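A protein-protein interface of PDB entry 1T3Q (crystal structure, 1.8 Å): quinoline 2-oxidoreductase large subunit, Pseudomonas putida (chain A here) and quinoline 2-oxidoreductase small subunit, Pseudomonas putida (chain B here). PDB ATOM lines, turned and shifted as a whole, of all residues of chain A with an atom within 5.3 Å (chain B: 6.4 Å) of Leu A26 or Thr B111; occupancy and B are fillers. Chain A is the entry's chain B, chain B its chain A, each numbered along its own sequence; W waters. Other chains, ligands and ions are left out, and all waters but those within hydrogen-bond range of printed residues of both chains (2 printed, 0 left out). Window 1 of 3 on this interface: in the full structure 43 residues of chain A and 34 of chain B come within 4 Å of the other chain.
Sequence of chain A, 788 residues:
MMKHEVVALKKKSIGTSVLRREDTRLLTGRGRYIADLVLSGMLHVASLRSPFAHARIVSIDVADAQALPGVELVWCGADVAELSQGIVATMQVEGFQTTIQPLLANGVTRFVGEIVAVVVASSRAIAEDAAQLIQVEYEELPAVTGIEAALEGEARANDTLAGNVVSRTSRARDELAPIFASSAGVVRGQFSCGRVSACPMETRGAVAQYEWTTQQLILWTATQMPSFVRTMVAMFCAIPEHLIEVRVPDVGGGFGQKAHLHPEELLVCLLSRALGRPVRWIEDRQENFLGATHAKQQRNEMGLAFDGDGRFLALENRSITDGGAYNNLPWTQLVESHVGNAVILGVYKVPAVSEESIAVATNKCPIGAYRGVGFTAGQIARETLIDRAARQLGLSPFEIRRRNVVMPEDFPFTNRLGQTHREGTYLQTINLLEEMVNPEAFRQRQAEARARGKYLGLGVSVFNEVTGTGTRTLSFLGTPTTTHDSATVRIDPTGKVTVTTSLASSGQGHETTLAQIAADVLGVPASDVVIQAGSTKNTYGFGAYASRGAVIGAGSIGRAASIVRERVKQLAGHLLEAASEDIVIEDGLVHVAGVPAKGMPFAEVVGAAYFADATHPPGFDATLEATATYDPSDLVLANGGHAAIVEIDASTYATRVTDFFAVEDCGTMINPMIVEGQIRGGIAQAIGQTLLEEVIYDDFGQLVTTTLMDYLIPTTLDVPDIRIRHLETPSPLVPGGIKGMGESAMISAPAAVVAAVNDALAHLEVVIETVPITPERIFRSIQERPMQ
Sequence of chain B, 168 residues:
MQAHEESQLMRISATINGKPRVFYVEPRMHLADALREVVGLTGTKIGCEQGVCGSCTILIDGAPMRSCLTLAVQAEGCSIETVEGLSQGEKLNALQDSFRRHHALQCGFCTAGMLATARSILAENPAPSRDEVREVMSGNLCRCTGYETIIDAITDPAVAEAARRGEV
NH1 of Arg A20 sits at hydrogen-bond distance from O of Gln B106 (2.7 Å).
OH of Tyr A33 sits at hydrogen-bond distance from O of Cys B107 (2.6 Å).
The backbone carbonyl oxygen (O) of Leu B105 lies within hydrogen-bond range of the guanidinium group (NH1) of Arg A20 (3.3 Å).
The backbone carbonyl oxygen (O) of Gly B108 lies close to the side-chain hydroxyl (OH) of Tyr A33 (3.4 Å).
N of Phe B109 lies within hydrogen-bond range of OH of Tyr A33.
OG1 of Thr B111 sits at hydrogen-bond distance from O of Gly B108 (3.2 Å).
OD1 of Asp A23 is in salt-bridge range of NE of Arg A20 (2.7 Å).
NH2 of Arg A20 lies within salt-bridge range of OE2 of Glu A22, at 3.7 Å.
The side-chain sulfur (SG) of Cys B107 lies close to the backbone NH (N) of Phe B109 (3.3 Å).
O of Phe B99 sits at hydrogen-bond distance from N of Ala B104 (2.8 Å).
Among the printed residues, merely in contact across the chains: Asp A23 with Leu B105 (3.7 Å), Leu A26 with Leu B105 (3.6 Å), Leu A26 with Gln B106 (3.9 Å), Leu A26 with Cys B107 (3.9 Å), Leu A26 with Thr B111 (3.8 Å), Leu A27 with Val B83 (3.4 Å), Leu A27 with Phe B99 (3.5 Å), Leu A27 with Thr B111 (3.5 Å), Leu A27 with Leu B115 (3.6 Å) and Gly A29 with Val B83 (3.5 Å).
Printed residues of chain B within 4 Å of Arg A20: Leu B105 and Gln B106.
Leu A26 touches just these residues of chain B: Leu B105 (3.6 Å), Gln B106 (3.9 Å), Cys B107 (3.9 Å) and Thr B111 (3.8 Å).
Printed residues of chain B within 4 Å of Leu A27: Val B83, Phe B99, Thr B111 and Leu B115.
Of the printed residues of chain B, Gly A29 touches Val B83.
Arg A30 touches none of the printed residues of chain B.
Of the printed residues of chain A, Gln B106 touches Arg A20 and Leu A26.
Thr B111 touches two residues of chain A.
The nearest residue of chain B that does not touch Leu A26 is Gly B108 (4.2 Å).
The nearest printed residue of chain A that does not touch Thr B111 is Tyr A33 (6.2 Å).
Printed residues of chain B that touch a printed residue of chain A: Val B83, Phe B99, Leu B105, Gln B106, Cys B107, Gly B108, Phe B109, Thr B111 and Leu B115.
Printed residues of chain A that touch a printed residue of chain B: Arg A20, Asp A23, Leu A26, Leu A27, Gly A29 and Tyr A33.
Hydrophobic or aromatic side chains of chain A within 4 Å of the printed part of chain B: Leu A26, Leu A27 and Tyr A33.
Among the printed residues, 15 pairs touch across the chains.
Water W1 bridges OD2 of Asp A23 (2.6 Å) and O of Leu B105 (2.8 Å).
Water W2 lies within hydrogen-bond range of the backbone carbonyl oxygen of Leu A26 (2.7 Å), the backbone carbonyl oxygen of Gly B108 (3.0 Å) and the side-chain hydroxyl of Tyr A33 (3.2 Å).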
ATOM      1  N   ARG A  20       6.050  12.504 -16.285  1.00  0.00           N
ATOM      2  CA  ARG A  20       5.680  12.727 -14.891  1.00  0.00           C
ATOM      3  C   ARG A  20       4.325  12.169 -14.483  1.00  0.00           C
ATOM      4  O   ARG A  20       3.305  12.464 -15.096  1.00  0.00           O
ATOM      5  CB  ARG A  20       5.742  14.224 -14.567  1.00  0.00           C
ATOM      6  CG  ARG A  20       7.065  14.880 -14.941  1.00  0.00           C
ATOM      7  CD  ARG A  20       7.299  16.134 -14.113  1.00  0.00           C
ATOM      8  NE  ARG A  20       6.058  16.886 -13.940  1.00  0.00           N
ATOM      9  CZ  ARG A  20       5.884  17.841 -13.037  1.00  0.00           C
ATOM     10  NH1 ARG A  20       4.714  18.463 -12.948  1.00  0.00           N
ATOM     11  NH2 ARG A  20       6.881  18.174 -12.226  1.00  0.00           N
ATOM     12  N   GLU A  22       2.730  12.945 -11.818  1.00  0.00           N
ATOM     13  CA  GLU A  22       1.907  13.973 -11.188  1.00  0.00           C
ATOM     14  C   GLU A  22       1.153  14.859 -12.179  1.00  0.00           C
ATOM     15  O   GLU A  22       0.166  15.501 -11.817  1.00  0.00           O
ATOM     16  CB  GLU A  22       2.751  14.855 -10.255  1.00  0.00           C
ATOM     17  CG  GLU A  22       3.951  15.517 -10.898  1.00  0.00           C
ATOM     18  CD  GLU A  22       5.235  14.723 -10.701  1.00  0.00           C
ATOM     19  OE1 GLU A  22       5.296  13.558 -11.148  1.00  0.00           O
ATOM     20  OE2 GLU A  22       6.186  15.265 -10.091  1.00  0.00           O
ATOM     21  N   ASP A  23       1.605  14.882 -13.430  1.00  0.00           N
ATOM     22  CA  ASP A  23       0.985  15.721 -14.454  1.00  0.00           C
ATOM     23  C   ASP A  23      -0.504  15.519 -14.668  1.00  0.00           C
ATOM     24  O   ASP A  23      -1.226  16.483 -14.906  1.00  0.00           O
ATOM     25  CB  ASP A  23       1.685  15.534 -15.804  1.00  0.00           C
ATOM     26  CG  ASP A  23       3.035  16.219 -15.872  1.00  0.00           C
ATOM     27  OD1 ASP A  23       3.487  16.786 -14.850  1.00  0.00           O
ATOM     28  OD2 ASP A  23       3.651  16.187 -16.957  1.00  0.00           O
ATOM     29  N   THR A  24      -0.970  14.277 -14.584  1.00  0.00           N
ATOM     30  CA  THR A  24      -2.376  14.007 -14.844  1.00  0.00           C
ATOM     31  C   THR A  24      -3.333  14.721 -13.897  1.00  0.00           C
ATOM     32  O   THR A  24      -4.317  15.309 -14.344  1.00  0.00           O
ATOM     33  CB  THR A  24      -2.651  12.490 -14.859  1.00  0.00           C
ATOM     34  OG1 THR A  24      -1.789  11.876 -15.828  1.00  0.00           O
ATOM     35  CG2 THR A  24      -4.096  12.208 -15.256  1.00  0.00           C
ATOM     36  N   ARG A  25      -3.057  14.705 -12.599  1.00  0.00           N
ATOM     37  CA  ARG A  25      -3.959  15.404 -11.696  1.00  0.00           C
ATOM     38  C   ARG A  25      -3.777  16.917 -11.820  1.00  0.00           C
ATOM     39  O   ARG A  25      -4.728  17.680 -11.655  1.00  0.00           O
ATOM     40  CB  ARG A  25      -3.747  14.962 -10.238  1.00  0.00           C
ATOM     41  CG  ARG A  25      -2.450  15.406  -9.580  1.00  0.00           C
ATOM     42  CD  ARG A  25      -2.494  15.038  -8.084  1.00  0.00           C
ATOM     43  NE  ARG A  25      -1.256  15.345  -7.365  1.00  0.00           N
ATOM     44  CZ  ARG A  25      -0.128  14.646  -7.471  1.00  0.00           C
ATOM     45  NH1 ARG A  25      -0.069  13.590  -8.276  1.00  0.00           N
ATOM     46  NH2 ARG A  25       0.938  14.995  -6.755  1.00  0.00           N
ATOM     47  N   LEU A  26      -2.559  17.347 -12.131  1.00  0.00           N
ATOM     48  CA  LEU A  26      -2.257  18.770 -12.250  1.00  0.00           C
ATOM     49  C   LEU A  26      -2.771  19.411 -13.543  1.00  0.00           C
ATOM     50  O   LEU A  26      -2.804  20.634 -13.661  1.00  0.00           O
ATOM     51  CB  LEU A  26      -0.745  19.000 -12.116  1.00  0.00           C
ATOM     52  CG  LEU A  26      -0.111  18.527 -10.798  1.00  0.00           C
ATOM     53  CD1 LEU A  26       1.399  18.746 -10.852  1.00  0.00           C
ATOM     54  CD2 LEU A  26      -0.729  19.270  -9.613  1.00  0.00           C
ATOM     55  N   LEU A  27      -3.178  18.585 -14.503  1.00  0.00           N
ATOM     56  CA  LEU A  27      -3.696  19.082 -15.781  1.00  0.00           C
ATOM     57  C   LEU A  27      -5.219  19.012 -15.828  1.00  0.00           C
ATOM     58  O   LEU A  27      -5.847  19.538 -16.752  1.00  0.00           O
ATOM     59  CB  LEU A  27      -3.124  18.255 -16.944  1.00  0.00           C
ATOM     60  CG  LEU A  27      -1.697  18.536 -17.406  1.00  0.00           C
ATOM     61  CD1 LEU A  27      -1.131  17.318 -18.131  1.00  0.00           C
ATOM     62  CD2 LEU A  27      -1.696  19.760 -18.304  1.00  0.00           C
ATOM     63  N   THR A  28      -5.811  18.364 -14.831  1.00  0.00           N
ATOM     64  CA  THR A  28      -7.258  18.208 -14.779  1.00  0.00           C
ATOM     65  C   THR A  28      -7.920  18.968 -13.640  1.00  0.00           C
ATOM     66  O   THR A  28      -9.099  18.755 -13.350  1.00  0.00           O
ATOM     67  CB  THR A  28      -7.629  16.732 -14.643  1.00  0.00           C
ATOM     68  OG1 THR A  28      -6.952  16.178 -13.505  1.00  0.00           O
ATOM     69  CG2 THR A  28      -7.225  15.964 -15.907  1.00  0.00           C
ATOM     70  N   GLY A  29      -7.166  19.854 -12.999  1.00  0.00           N
ATOM     71  CA  GLY A  29      -7.717  20.619 -11.896  1.00  0.00           C
ATOM     72  C   GLY A  29      -7.852  19.787 -10.634  1.00  0.00           C
ATOM     73  O   GLY A  29      -8.549  20.177  -9.698  1.00  0.00           O
ATOM     74  N   ARG A  30      -7.176  18.644 -10.591  1.00  0.00           N
ATOM     75  CA  ARG A  30      -7.265  17.786  -9.421  1.00  0.00           C
ATOM     76  C   ARG A  30      -6.028  17.780  -8.524  1.00  0.00           C
ATOM     77  O   ARG A  30      -5.824  16.859  -7.731  1.00  0.00           O
ATOM     78  CB  ARG A  30      -7.625  16.367  -9.843  1.00  0.00           C
ATOM     79  CG  ARG A  30      -8.979  16.294 -10.528  1.00  0.00           C
ATOM     80  CD  ARG A  30      -9.530  14.886 -10.482  1.00  0.00           C
ATOM     81  NE  ARG A  30     -10.828  14.787 -11.138  1.00  0.00           N
ATOM     82  CZ  ARG A  30     -11.626  13.731 -11.044  1.00  0.00           C
ATOM     83  NH1 ARG A  30     -12.794  13.718 -11.676  1.00  0.00           N
ATOM     84  NH2 ARG A  30     -11.258  12.690 -10.309  1.00  0.00           N
ATOM     85  N   GLY A  31      -5.200  18.804  -8.664  1.00  0.00           N
ATOM     86  CA  GLY A  31      -4.039  18.909  -7.804  1.00  0.00           C
ATOM     87  C   GLY A  31      -4.653  19.352  -6.492  1.00  0.00           C
ATOM     88  O   GLY A  31      -5.758  19.889  -6.492  1.00  0.00           O
ATOM     89  N   TYR A  33      -3.684  21.716  -3.557  1.00  0.00           N
ATOM     90  CA  TYR A  33      -2.793  22.684  -2.929  1.00  0.00           C
ATOM     91  C   TYR A  33      -3.361  23.157  -1.588  1.00  0.00           C
ATOM     92  O   TYR A  33      -4.513  22.878  -1.255  1.00  0.00           O
ATOM     93  CB  TYR A  33      -2.555  23.870  -3.869  1.00  0.00           C
ATOM     94  CG  TYR A  33      -2.005  23.476  -5.230  1.00  0.00           C
ATOM     95  CD1 TYR A  33      -2.842  22.959  -6.222  1.00  0.00           C
ATOM     96  CD2 TYR A  33      -0.648  23.633  -5.530  1.00  0.00           C
ATOM     97  CE1 TYR A  33      -2.344  22.613  -7.485  1.00  0.00           C
ATOM     98  CE2 TYR A  33      -0.138  23.289  -6.786  1.00  0.00           C
ATOM     99  CZ  TYR A  33      -0.995  22.784  -7.760  1.00  0.00           C
ATOM    100  OH  TYR A  33      -0.505  22.487  -9.012  1.00  0.00           O
ATOM    101  N   ASP A 250       0.118  19.464  -2.547  1.00  0.00           N
ATOM    102  CA  ASP A 250       0.886  19.829  -3.728  1.00  0.00           C
ATOM    103  C   ASP A 250       1.239  21.291  -3.478  1.00  0.00           C
ATOM    104  O   ASP A 250       0.424  22.038  -2.935  1.00  0.00           O
ATOM    105  CB  ASP A 250       0.035  19.702  -4.997  1.00  0.00           C
ATOM    106  CG  ASP A 250      -0.240  18.254  -5.371  1.00  0.00           C
ATOM    107  OD1 ASP A 250       0.707  17.445  -5.296  1.00  0.00           O
ATOM    108  OD2 ASP A 250      -1.388  17.926  -5.756  1.00  0.00           O
ATOM    109  N   SER B  55      -3.638  33.065 -13.630  1.00  0.00           N
ATOM    110  CA  SER B  55      -3.880  31.736 -13.072  1.00  0.00           C
ATOM    111  C   SER B  55      -5.356  31.373 -12.909  1.00  0.00           C
ATOM    112  O   SER B  55      -5.695  30.193 -12.839  1.00  0.00           O
ATOM    113  CB  SER B  55      -3.193  31.590 -11.708  1.00  0.00           C
ATOM    114  OG  SER B  55      -3.895  32.321 -10.719  1.00  0.00           O
ATOM    115  N   VAL B  83     -11.090  24.138 -15.910  1.00  0.00           N
ATOM    116  CA  VAL B  83     -10.186  23.061 -16.286  1.00  0.00           C
ATOM    117  C   VAL B  83     -10.772  21.670 -16.031  1.00  0.00           C
ATOM    118  O   VAL B  83     -10.466  20.725 -16.761  1.00  0.00           O
ATOM    119  CB  VAL B  83      -8.832  23.195 -15.544  1.00  0.00           C
ATOM    120  CG1 VAL B  83      -9.031  23.013 -14.054  1.00  0.00           C
ATOM    121  CG2 VAL B  83      -7.840  22.177 -16.086  1.00  0.00           C
ATOM    122  N   PHE B  99       0.788  18.783 -23.160  1.00  0.00           N
ATOM    123  CA  PHE B  99       1.467  19.478 -22.062  1.00  0.00           C
ATOM    124  C   PHE B  99       2.347  18.476 -21.308  1.00  0.00           C
ATOM    125  O   PHE B  99       3.487  18.775 -20.945  1.00  0.00           O
ATOM    126  CB  PHE B  99       0.438  20.079 -21.088  1.00  0.00           C
ATOM    127  CG  PHE B  99       0.134  21.528 -21.339  1.00  0.00           C
ATOM    128  CD1 PHE B  99      -0.342  21.956 -22.579  1.00  0.00           C
ATOM    129  CD2 PHE B  99       0.320  22.471 -20.332  1.00  0.00           C
ATOM    130  CE1 PHE B  99      -0.627  23.298 -22.811  1.00  0.00           C
ATOM    131  CE2 PHE B  99       0.037  23.823 -20.555  1.00  0.00           C
ATOM    132  CZ  PHE B  99      -0.438  24.237 -21.795  1.00  0.00           C
ATOM    133  N   ALA B 104       5.327  20.601 -19.969  1.00  0.00           N
ATOM    134  CA  ALA B 104       4.896  21.996 -19.984  1.00  0.00           C
ATOM    135  C   ALA B 104       4.432  22.500 -18.613  1.00  0.00           C
ATOM    136  O   ALA B 104       3.881  23.590 -18.505  1.00  0.00           O
ATOM    137  CB  ALA B 104       3.772  22.183 -21.008  1.00  0.00           C
ATOM    138  N   LEU B 105       4.628  21.695 -17.577  1.00  0.00           N
ATOM    139  CA  LEU B 105       4.259  22.106 -16.223  1.00  0.00           C
ATOM    140  C   LEU B 105       5.188  21.456 -15.191  1.00  0.00           C
ATOM    141  O   LEU B 105       5.752  20.395 -15.419  1.00  0.00           O
ATOM    142  CB  LEU B 105       2.812  21.735 -15.887  1.00  0.00           C
ATOM    143  CG  LEU B 105       2.505  20.246 -15.818  1.00  0.00           C
ATOM    144  CD1 LEU B 105       1.367  19.989 -14.844  1.00  0.00           C
ATOM    145  CD2 LEU B 105       2.158  19.745 -17.220  1.00  0.00           C
ATOM    146  N   GLN B 106       5.323  22.127 -14.055  1.00  0.00           N
ATOM    147  CA  GLN B 106       6.137  21.674 -12.955  1.00  0.00           C
ATOM    148  C   GLN B 106       5.303  21.673 -11.671  1.00  0.00           C
ATOM    149  O   GLN B 106       4.777  20.623 -11.258  1.00  0.00           O
ATOM    150  CB  GLN B 106       7.391  22.554 -12.846  1.00  0.00           C
ATOM    151  CG  GLN B 106       8.484  22.141 -13.848  1.00  0.00           C
ATOM    152  CD  GLN B 106       9.786  22.928 -13.790  1.00  0.00           C
ATOM    153  OE1 GLN B 106      10.317  23.212 -12.719  1.00  0.00           O
ATOM    154  NE2 GLN B 106      10.320  23.257 -14.965  1.00  0.00           N
ATOM    155  N   CYS B 107       5.165  22.838 -11.049  1.00  0.00           N
ATOM    156  CA  CYS B 107       4.364  22.878  -9.830  1.00  0.00           C
ATOM    157  C   CYS B 107       2.894  22.743 -10.243  1.00  0.00           C
ATOM    158  O   CYS B 107       2.060  22.285  -9.469  1.00  0.00           O
ATOM    159  CB  CYS B 107       4.624  24.196  -9.100  1.00  0.00           C
ATOM    160  SG  CYS B 107       3.730  25.634  -9.696  1.00  0.00           S
ATOM    161  N   GLY B 108       2.609  23.147 -11.479  1.00  0.00           N
ATOM    162  CA  GLY B 108       1.257  23.044 -12.016  1.00  0.00           C
ATOM    163  C   GLY B 108       0.227  24.097 -11.631  1.00  0.00           C
ATOM    164  O   GLY B 108      -0.948  24.012 -12.023  1.00  0.00           O
ATOM    165  N   PHE B 109       0.654  25.112 -10.891  1.00  0.00           N
ATOM    166  CA  PHE B 109      -0.279  26.140 -10.443  1.00  0.00           C
ATOM    167  C   PHE B 109      -0.832  27.037 -11.553  1.00  0.00           C
ATOM    168  O   PHE B 109      -1.977  27.480 -11.486  1.00  0.00           O
ATOM    169  CB  PHE B 109       0.382  27.004  -9.371  1.00  0.00           C
ATOM    170  CG  PHE B 109      -0.595  27.614  -8.414  1.00  0.00           C
ATOM    171  CD1 PHE B 109      -1.303  26.809  -7.530  1.00  0.00           C
ATOM    172  CD2 PHE B 109      -0.814  28.986  -8.395  1.00  0.00           C
ATOM    173  CE1 PHE B 109      -2.225  27.366  -6.627  1.00  0.00           C
ATOM    174  CE2 PHE B 109      -1.732  29.551  -7.497  1.00  0.00           C
ATOM    175  CZ  PHE B 109      -2.435  28.734  -6.614  1.00  0.00           C
ATOM    176  N   CYS B 110      -0.027  27.285 -12.579  1.00  0.00           N
ATOM    177  CA  CYS B 110      -0.434  28.145 -13.693  1.00  0.00           C
ATOM    178  C   CYS B 110      -1.137  27.368 -14.797  1.00  0.00           C
ATOM    179  O   CYS B 110      -1.695  27.959 -15.717  1.00  0.00           O
ATOM    180  CB  CYS B 110       0.793  28.786 -14.318  1.00  0.00           C
ATOM    181  SG  CYS B 110       1.811  27.567 -15.235  1.00  0.00           S
ATOM    182  N   THR B 111      -1.108  26.047 -14.691  1.00  0.00           N
ATOM    183  CA  THR B 111      -1.650  25.187 -15.732  1.00  0.00           C
ATOM    184  C   THR B 111      -3.108  25.388 -16.137  1.00  0.00           C
ATOM    185  O   THR B 111      -3.402  25.459 -17.329  1.00  0.00           O
ATOM    186  CB  THR B 111      -1.371  23.719 -15.371  1.00  0.00           C
ATOM    187  OG1 THR B 111       0.021  23.591 -15.043  1.00  0.00           O
ATOM    188  CG2 THR B 111      -1.660  22.803 -16.553  1.00  0.00           C
ATOM    189  N   ALA B 112      -4.017  25.485 -15.176  1.00  0.00           N
ATOM    190  CA  ALA B 112      -5.425  25.702 -15.519  1.00  0.00           C
ATOM    191  C   ALA B 112      -5.575  26.953 -16.401  1.00  0.00           C
ATOM    192  O   ALA B 112      -6.249  26.923 -17.440  1.00  0.00           O
ATOM    193  CB  ALA B 112      -6.261  25.835 -14.251  1.00  0.00           C
ATOM    194  N   GLY B 113      -4.936  28.047 -15.997  1.00  0.00           N
ATOM    195  CA  GLY B 113      -5.002  29.279 -16.768  1.00  0.00           C
ATOM    196  C   GLY B 113      -4.347  29.158 -18.135  1.00  0.00           C
ATOM    197  O   GLY B 113      -4.851  29.704 -19.122  1.00  0.00           O
ATOM    198  N   MET B 114      -3.219  28.450 -18.196  1.00  0.00           N
ATOM    199  CA  MET B 114      -2.509  28.239 -19.453  1.00  0.00           C
ATOM    200  C   MET B 114      -3.422  27.535 -20.453  1.00  0.00           C
ATOM    201  O   MET B 114      -3.525  27.946 -21.605  1.00  0.00           O
ATOM    202  CB  MET B 114      -1.265  27.370 -19.231  1.00  0.00           C
ATOM    203  CG  MET B 114      -0.114  28.064 -18.527  1.00  0.00           C
ATOM    204  SD  MET B 114       0.571  29.383 -19.521  1.00  0.00           S
ATOM    205  CE  MET B 114       1.629  30.205 -18.270  1.00  0.00           C
ATOM    206  N   LEU B 115      -4.078  26.473 -19.999  1.00  0.00           N
ATOM    207  CA  LEU B 115      -4.974  25.694 -20.850  1.00  0.00           C
ATOM    208  C   LEU B 115      -6.140  26.511 -21.403  1.00  0.00           C
ATOM    209  O   LEU B 115      -6.516  26.360 -22.574  1.00  0.00           O
ATOM    210  CB  LEU B 115      -5.502  24.477 -20.079  1.00  0.00           C
ATOM    211  CG  LEU B 115      -4.457  23.404 -19.739  1.00  0.00           C
ATOM    212  CD1 LEU B 115      -5.031  22.412 -18.741  1.00  0.00           C
ATOM    213  CD2 LEU B 115      -4.018  22.693 -21.012  1.00  0.00           C
ATOM    214  N   ALA B 116      -6.708  27.378 -20.566  1.00  0.00           N
ATOM    215  CA  ALA B 116      -7.826  28.218 -20.984  1.00  0.00           C
ATOM    216  C   ALA B 116      -7.394  29.115 -22.144  1.00  0.00           C
ATOM    217  O   ALA B 116      -8.046  29.159 -23.193  1.00  0.00           O
ATOM    218  CB  ALA B 116      -8.318  29.073 -19.799  1.00  0.00           C
HETATM  219  O   HOH W   1       5.175  18.315 -17.275  1.00  0.00           O
HETATM  220  O   HOH W   2      -2.758  21.726 -11.140  1.00  0.00           O
